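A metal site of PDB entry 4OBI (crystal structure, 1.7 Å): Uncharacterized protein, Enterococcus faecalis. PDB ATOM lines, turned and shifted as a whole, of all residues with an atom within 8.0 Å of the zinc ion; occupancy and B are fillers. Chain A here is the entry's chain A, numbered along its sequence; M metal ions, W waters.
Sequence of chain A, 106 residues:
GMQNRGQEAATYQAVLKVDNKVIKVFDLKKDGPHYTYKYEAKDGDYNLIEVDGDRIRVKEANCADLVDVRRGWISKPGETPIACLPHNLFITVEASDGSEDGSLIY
The zinc ion is bound by water W1 (2.0 Å), the side-chain carboxylate (OD1) of Asp 68 (2.0 Å), the side-chain sulfur (SG) of Cys 63 (2.3 Å) and the side-chain sulfur (SG) of Cys 84 (2.3 Å).
The side-chain sulfur (SG) of Cys 84 lies close to the side-chain amide nitrogen (ND2) of Asn 47, at 3.4 Å.
The backbone NH (N) of Cys 84 lies within hydrogen-bond range of the backbone carbonyl oxygen (O) of Leu 89, at 2.8 Å.
ND1 of His 87 sits close to SG of Cys 84.
ND2 of Asn 47 is in hydrogen-bond range of OD2 of Asp 68, 2.9 Å away.
The side-chain sulfur of Cys 63 sits close to the backbone NH of Leu 66 (3.4 Å).
Of the 22 residues printed, 3 come within 4 Å of the zinc ion.
The nearest printed residue that does not touch the zinc ion is Asp 65 (4.01 Å).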
ATOM      1  N   TYR A  46     -17.566   4.628  18.800  1.00  0.00           N
ATOM      2  CA  TYR A  46     -16.411   5.482  18.996  1.00  0.00           C
ATOM      3  C   TYR A  46     -16.094   6.350  17.791  1.00  0.00           C
ATOM      4  O   TYR A  46     -16.468   6.048  16.659  1.00  0.00           O
ATOM      5  CB  TYR A  46     -15.178   4.656  19.392  1.00  0.00           C
ATOM      6  CG  TYR A  46     -14.431   4.030  18.237  1.00  0.00           C
ATOM      7  CD1 TYR A  46     -14.819   2.812  17.722  1.00  0.00           C
ATOM      8  CD2 TYR A  46     -13.317   4.651  17.677  1.00  0.00           C
ATOM      9  CE1 TYR A  46     -14.134   2.222  16.666  1.00  0.00           C
ATOM     10  CE2 TYR A  46     -12.627   4.078  16.620  1.00  0.00           C
ATOM     11  CZ  TYR A  46     -13.047   2.864  16.114  1.00  0.00           C
ATOM     12  OH  TYR A  46     -12.371   2.271  15.061  1.00  0.00           O
ATOM     13  N   ASN A  47     -15.407   7.458  18.095  1.00  0.00           N
ATOM     14  CA  ASN A  47     -14.884   8.379  17.104  1.00  0.00           C
ATOM     15  C   ASN A  47     -13.550   8.838  17.627  1.00  0.00           C
ATOM     16  O   ASN A  47     -13.454   9.262  18.789  1.00  0.00           O
ATOM     17  CB  ASN A  47     -15.773   9.586  16.932  1.00  0.00           C
ATOM     18  CG  ASN A  47     -17.184   9.220  16.565  1.00  0.00           C
ATOM     19  OD1 ASN A  47     -17.955   8.786  17.411  1.00  0.00           O
ATOM     20  ND2 ASN A  47     -17.539   9.409  15.308  1.00  0.00           N
ATOM     21  N   VAL A  58     -12.043  13.914  12.503  1.00  0.00           N
ATOM     22  CA  VAL A  58     -12.275  12.565  13.001  1.00  0.00           C
ATOM     23  C   VAL A  58     -11.435  11.642  12.110  1.00  0.00           C
ATOM     24  O   VAL A  58     -11.674  11.556  10.913  1.00  0.00           O
ATOM     25  CB  VAL A  58     -13.759  12.169  12.963  1.00  0.00           C
ATOM     26  CG1 VAL A  58     -13.933  10.729  13.436  1.00  0.00           C
ATOM     27  CG2 VAL A  58     -14.581  13.122  13.842  1.00  0.00           C
ATOM     28  N   GLU A  60     -10.913   8.288  12.611  1.00  0.00           N
ATOM     29  CA  GLU A  60     -11.369   6.913  12.591  1.00  0.00           C
ATOM     30  C   GLU A  60     -12.667   6.851  13.372  1.00  0.00           C
ATOM     31  O   GLU A  60     -12.862   7.620  14.327  1.00  0.00           O
ATOM     32  CB  GLU A  60     -10.287   6.026  13.235  1.00  0.00           C
ATOM     33  CG  GLU A  60     -10.576   4.539  13.240  1.00  0.00           C
ATOM     34  CD  GLU A  60      -9.519   3.731  13.973  1.00  0.00           C
ATOM     35  OE1 GLU A  60      -8.310   4.041  13.823  1.00  0.00           O
ATOM     36  OE2 GLU A  60      -9.887   2.778  14.691  1.00  0.00           O
ATOM     37  N   ALA A  61     -13.563   5.947  12.976  1.00  0.00           N
ATOM     38  CA  ALA A  61     -14.844   5.742  13.670  1.00  0.00           C
ATOM     39  C   ALA A  61     -15.459   4.398  13.284  1.00  0.00           C
ATOM     40  O   ALA A  61     -14.997   3.777  12.329  1.00  0.00           O
ATOM     41  CB  ALA A  61     -15.804   6.875  13.347  1.00  0.00           C
ATOM     42  N   ASN A  62     -16.484   3.968  14.012  1.00  0.00           N
ATOM     43  CA  ASN A  62     -17.203   2.718  13.687  1.00  0.00           C
ATOM     44  C   ASN A  62     -18.701   2.897  13.476  1.00  0.00           C
ATOM     45  O   ASN A  62     -19.470   1.966  13.655  1.00  0.00           O
ATOM     46  CB  ASN A  62     -16.956   1.638  14.750  1.00  0.00           C
ATOM     47  CG  ASN A  62     -17.504   2.017  16.102  1.00  0.00           C
ATOM     48  OD1 ASN A  62     -17.978   3.139  16.325  1.00  0.00           O
ATOM     49  ND2 ASN A  62     -17.434   1.080  17.034  1.00  0.00           N
ATOM     50  N   CYS A  63     -19.092   4.105  13.081  1.00  0.00           N
ATOM     51  CA  CYS A  63     -20.448   4.336  12.617  1.00  0.00           C
ATOM     52  C   CYS A  63     -20.637   3.654  11.266  1.00  0.00           C
ATOM     53  O   CYS A  63     -19.678   3.238  10.627  1.00  0.00           O
ATOM     54  CB  CYS A  63     -20.719   5.823  12.500  1.00  0.00           C
ATOM     55  SG  CYS A  63     -19.544   6.669  11.426  1.00  0.00           S
ATOM     56  N   ALA A  64     -21.890   3.557  10.828  1.00  0.00           N
ATOM     57  CA  ALA A  64     -22.212   2.779   9.623  1.00  0.00           C
ATOM     58  C   ALA A  64     -21.807   3.435   8.302  1.00  0.00           C
ATOM     59  O   ALA A  64     -21.668   2.726   7.305  1.00  0.00           O
ATOM     60  CB  ALA A  64     -23.692   2.456   9.614  1.00  0.00           C
ATOM     61  N   ASP A  65     -21.645   4.757   8.265  1.00  0.00           N
ATOM     62  CA  ASP A  65     -21.358   5.450   7.001  1.00  0.00           C
ATOM     63  C   ASP A  65     -20.028   6.194   6.940  1.00  0.00           C
ATOM     64  O   ASP A  65     -19.613   6.654   5.871  1.00  0.00           O
ATOM     65  CB  ASP A  65     -22.506   6.398   6.634  1.00  0.00           C
ATOM     66  CG  ASP A  65     -22.780   7.450   7.711  1.00  0.00           C
ATOM     67  OD1 ASP A  65     -21.882   7.740   8.539  1.00  0.00           O
ATOM     68  OD2 ASP A  65     -23.912   7.987   7.731  1.00  0.00           O
ATOM     69  N   LEU A  66     -19.343   6.313   8.084  1.00  0.00           N
ATOM     70  CA  LEU A  66     -18.055   7.027   8.182  1.00  0.00           C
ATOM     71  C   LEU A  66     -18.081   8.430   7.575  1.00  0.00           C
ATOM     72  O   LEU A  66     -17.059   8.948   7.143  1.00  0.00           O
ATOM     73  CB  LEU A  66     -16.927   6.182   7.593  1.00  0.00           C
ATOM     74  CG  LEU A  66     -16.703   4.787   8.173  1.00  0.00           C
ATOM     75  CD1 LEU A  66     -15.538   4.099   7.487  1.00  0.00           C
ATOM     76  CD2 LEU A  66     -16.482   4.863   9.684  1.00  0.00           C
ATOM     77  N   VAL A  67     -19.244   9.071   7.583  1.00  0.00           N
ATOM     78  CA  VAL A  67     -19.394  10.392   6.937  1.00  0.00           C
ATOM     79  C   VAL A  67     -18.445  11.430   7.576  1.00  0.00           C
ATOM     80  O   VAL A  67     -17.793  12.208   6.863  1.00  0.00           O
ATOM     81  CB  VAL A  67     -20.872  10.840   6.944  1.00  0.00           C
ATOM     82  CG1 VAL A  67     -21.011  12.353   6.782  1.00  0.00           C
ATOM     83  CG2 VAL A  67     -21.632  10.131   5.836  1.00  0.00           C
ATOM     84  N   ASP A  68     -18.360  11.400   8.897  1.00  0.00           N
ATOM     85  CA  ASP A  68     -17.480  12.314   9.643  1.00  0.00           C
ATOM     86  C   ASP A  68     -16.013  12.070   9.310  1.00  0.00           C
ATOM     87  O   ASP A  68     -15.248  13.014   9.133  1.00  0.00           O
ATOM     88  CB  ASP A  68     -17.734  12.272  11.149  1.00  0.00           C
ATOM     89  CG  ASP A  68     -17.777  10.867  11.703  1.00  0.00           C
ATOM     90  OD1 ASP A  68     -18.486  10.012  11.137  1.00  0.00           O
ATOM     91  OD2 ASP A  68     -17.104  10.614  12.721  1.00  0.00           O
ATOM     92  N   VAL A  69     -15.609  10.807   9.209  1.00  0.00           N
ATOM     93  CA  VAL A  69     -14.259  10.462   8.761  1.00  0.00           C
ATOM     94  C   VAL A  69     -13.998  10.983   7.340  1.00  0.00           C
ATOM     95  O   VAL A  69     -12.923  11.556   7.048  1.00  0.00           O
ATOM     96  CB  VAL A  69     -14.018   8.932   8.834  1.00  0.00           C
ATOM     97  CG1 VAL A  69     -12.674   8.548   8.233  1.00  0.00           C
ATOM     98  CG2 VAL A  69     -14.081   8.452  10.266  1.00  0.00           C
ATOM     99  N   ARG A  70     -14.959  10.791   6.450  1.00  0.00           N
ATOM    100  CA  ARG A  70     -14.778  11.143   5.042  1.00  0.00           C
ATOM    101  C   ARG A  70     -14.735  12.662   4.828  1.00  0.00           C
ATOM    102  O   ARG A  70     -14.129  13.129   3.867  1.00  0.00           O
ATOM    103  CB  ARG A  70     -15.870  10.492   4.191  1.00  0.00           C
ATOM    104  CG  ARG A  70     -15.745   8.974   4.143  1.00  0.00           C
ATOM    105  CD  ARG A  70     -17.104   8.323   3.949  1.00  0.00           C
ATOM    106  NE  ARG A  70     -17.725   8.744   2.705  1.00  0.00           N
ATOM    107  CZ  ARG A  70     -19.007   8.586   2.399  1.00  0.00           C
ATOM    108  NH1 ARG A  70     -19.843   8.009   3.263  1.00  0.00           N
ATOM    109  NH2 ARG A  70     -19.457   9.025   1.239  1.00  0.00           N
ATOM    110  N   ILE A  82     -18.212  19.163  11.578  1.00  0.00           N
ATOM    111  CA  ILE A  82     -18.073  17.713  11.431  1.00  0.00           C
ATOM    112  C   ILE A  82     -19.198  17.099  12.237  1.00  0.00           C
ATOM    113  O   ILE A  82     -19.398  17.433  13.401  1.00  0.00           O
ATOM    114  CB  ILE A  82     -16.732  17.178  11.961  1.00  0.00           C
ATOM    115  CG1 ILE A  82     -15.575  17.745  11.131  1.00  0.00           C
ATOM    116  CG2 ILE A  82     -16.714  15.668  11.930  1.00  0.00           C
ATOM    117  CD1 ILE A  82     -14.213  17.672  11.816  1.00  0.00           C
ATOM    118  N   ALA A  83     -19.949  16.216  11.602  1.00  0.00           N
ATOM    119  CA  ALA A  83     -21.067  15.583  12.251  1.00  0.00           C
ATOM    120  C   ALA A  83     -21.034  14.065  12.068  1.00  0.00           C
ATOM    121  O   ALA A  83     -20.931  13.568  10.937  1.00  0.00           O
ATOM    122  CB  ALA A  83     -22.367  16.154  11.717  1.00  0.00           C
ATOM    123  N   CYS A  84     -21.135  13.358  13.191  1.00  0.00           N
ATOM    124  CA  CYS A  84     -21.427  11.931  13.183  1.00  0.00           C
ATOM    125  C   CYS A  84     -22.827  11.762  13.734  1.00  0.00           C
ATOM    126  O   CYS A  84     -23.034  11.632  14.946  1.00  0.00           O
ATOM    127  CB  CYS A  84     -20.419  11.156  14.018  1.00  0.00           C
ATOM    128  SG  CYS A  84     -20.703   9.369  13.967  1.00  0.00           S
ATOM    129  N   LEU A  85     -23.804  11.797  12.844  1.00  0.00           N
ATOM    130  CA  LEU A  85     -25.188  11.729  13.267  1.00  0.00           C
ATOM    131  C   LEU A  85     -25.552  10.415  14.009  1.00  0.00           C
ATOM    132  O   LEU A  85     -26.258  10.466  15.005  1.00  0.00           O
ATOM    133  CB  LEU A  85     -26.133  12.013  12.106  1.00  0.00           C
ATOM    134  CG  LEU A  85     -25.978  13.391  11.447  1.00  0.00           C
ATOM    135  CD1 LEU A  85     -26.955  13.516  10.278  1.00  0.00           C
ATOM    136  CD2 LEU A  85     -26.163  14.510  12.455  1.00  0.00           C
ATOM    137  N   PRO A  86     -25.033   9.251  13.545  1.00  0.00           N
ATOM    138  CA  PRO A  86     -25.315   8.004  14.271  1.00  0.00           C
ATOM    139  C   PRO A  86     -24.837   7.998  15.731  1.00  0.00           C
ATOM    140  O   PRO A  86     -25.476   7.369  16.567  1.00  0.00           O
ATOM    141  CB  PRO A  86     -24.559   6.941  13.447  1.00  0.00           C
ATOM    142  CG  PRO A  86     -24.440   7.536  12.089  1.00  0.00           C
ATOM    143  CD  PRO A  86     -24.239   8.999  12.330  1.00  0.00           C
ATOM    144  N   HIS A  87     -23.755   8.711  16.034  1.00  0.00           N
ATOM    145  CA  HIS A  87     -23.237   8.796  17.402  1.00  0.00           C
ATOM    146  C   HIS A  87     -23.654  10.087  18.118  1.00  0.00           C
ATOM    147  O   HIS A  87     -23.264  10.325  19.267  1.00  0.00           O
ATOM    148  CB  HIS A  87     -21.726   8.659  17.404  1.00  0.00           C
ATOM    149  CG  HIS A  87     -21.235   7.322  16.931  1.00  0.00           C
ATOM    150  ND1 HIS A  87     -19.900   7.047  16.753  1.00  0.00           N
ATOM    151  CD2 HIS A  87     -21.903   6.195  16.592  1.00  0.00           C
ATOM    152  CE1 HIS A  87     -19.763   5.807  16.316  1.00  0.00           C
ATOM    153  NE2 HIS A  87     -20.969   5.263  16.219  1.00  0.00           N
ATOM    154  N   ASN A  88     -24.453  10.921  17.437  1.00  0.00           N
ATOM    155  CA  ASN A  88     -24.889  12.210  17.967  1.00  0.00           C
ATOM    156  C   ASN A  88     -23.700  13.085  18.426  1.00  0.00           C
ATOM    157  O   ASN A  88     -23.729  13.678  19.516  1.00  0.00           O
ATOM    158  CB  ASN A  88     -25.877  12.002  19.114  1.00  0.00           C
ATOM    159  CG  ASN A  88     -26.818  13.169  19.294  1.00  0.00           C
ATOM    160  OD1 ASN A  88     -26.923  14.036  18.423  1.00  0.00           O
ATOM    161  ND2 ASN A  88     -27.538  13.195  20.404  1.00  0.00           N
ATOM    162  N   LEU A  89     -22.682  13.136  17.578  1.00  0.00           N
ATOM    163  CA  LEU A  89     -21.421  13.798  17.867  1.00  0.00           C
ATOM    164  C   LEU A  89     -21.137  14.886  16.828  1.00  0.00           C
ATOM    165  O   LEU A  89     -21.341  14.669  15.627  1.00  0.00           O
ATOM    166  CB  LEU A  89     -20.295  12.777  17.871  1.00  0.00           C
ATOM    167  CG  LEU A  89     -18.841  13.279  18.014  1.00  0.00           C
ATOM    168  CD1 LEU A  89     -18.001  12.237  18.732  1.00  0.00           C
ATOM    169  CD2 LEU A  89     -18.184  13.665  16.699  1.00  0.00           C
HETATM  170 ZN    ZN M   1     -19.959   8.849  11.880  1.00  0.00          ZN
HETATM  171  O   HOH W   1     -21.266   9.345  10.480  1.00  0.00           O
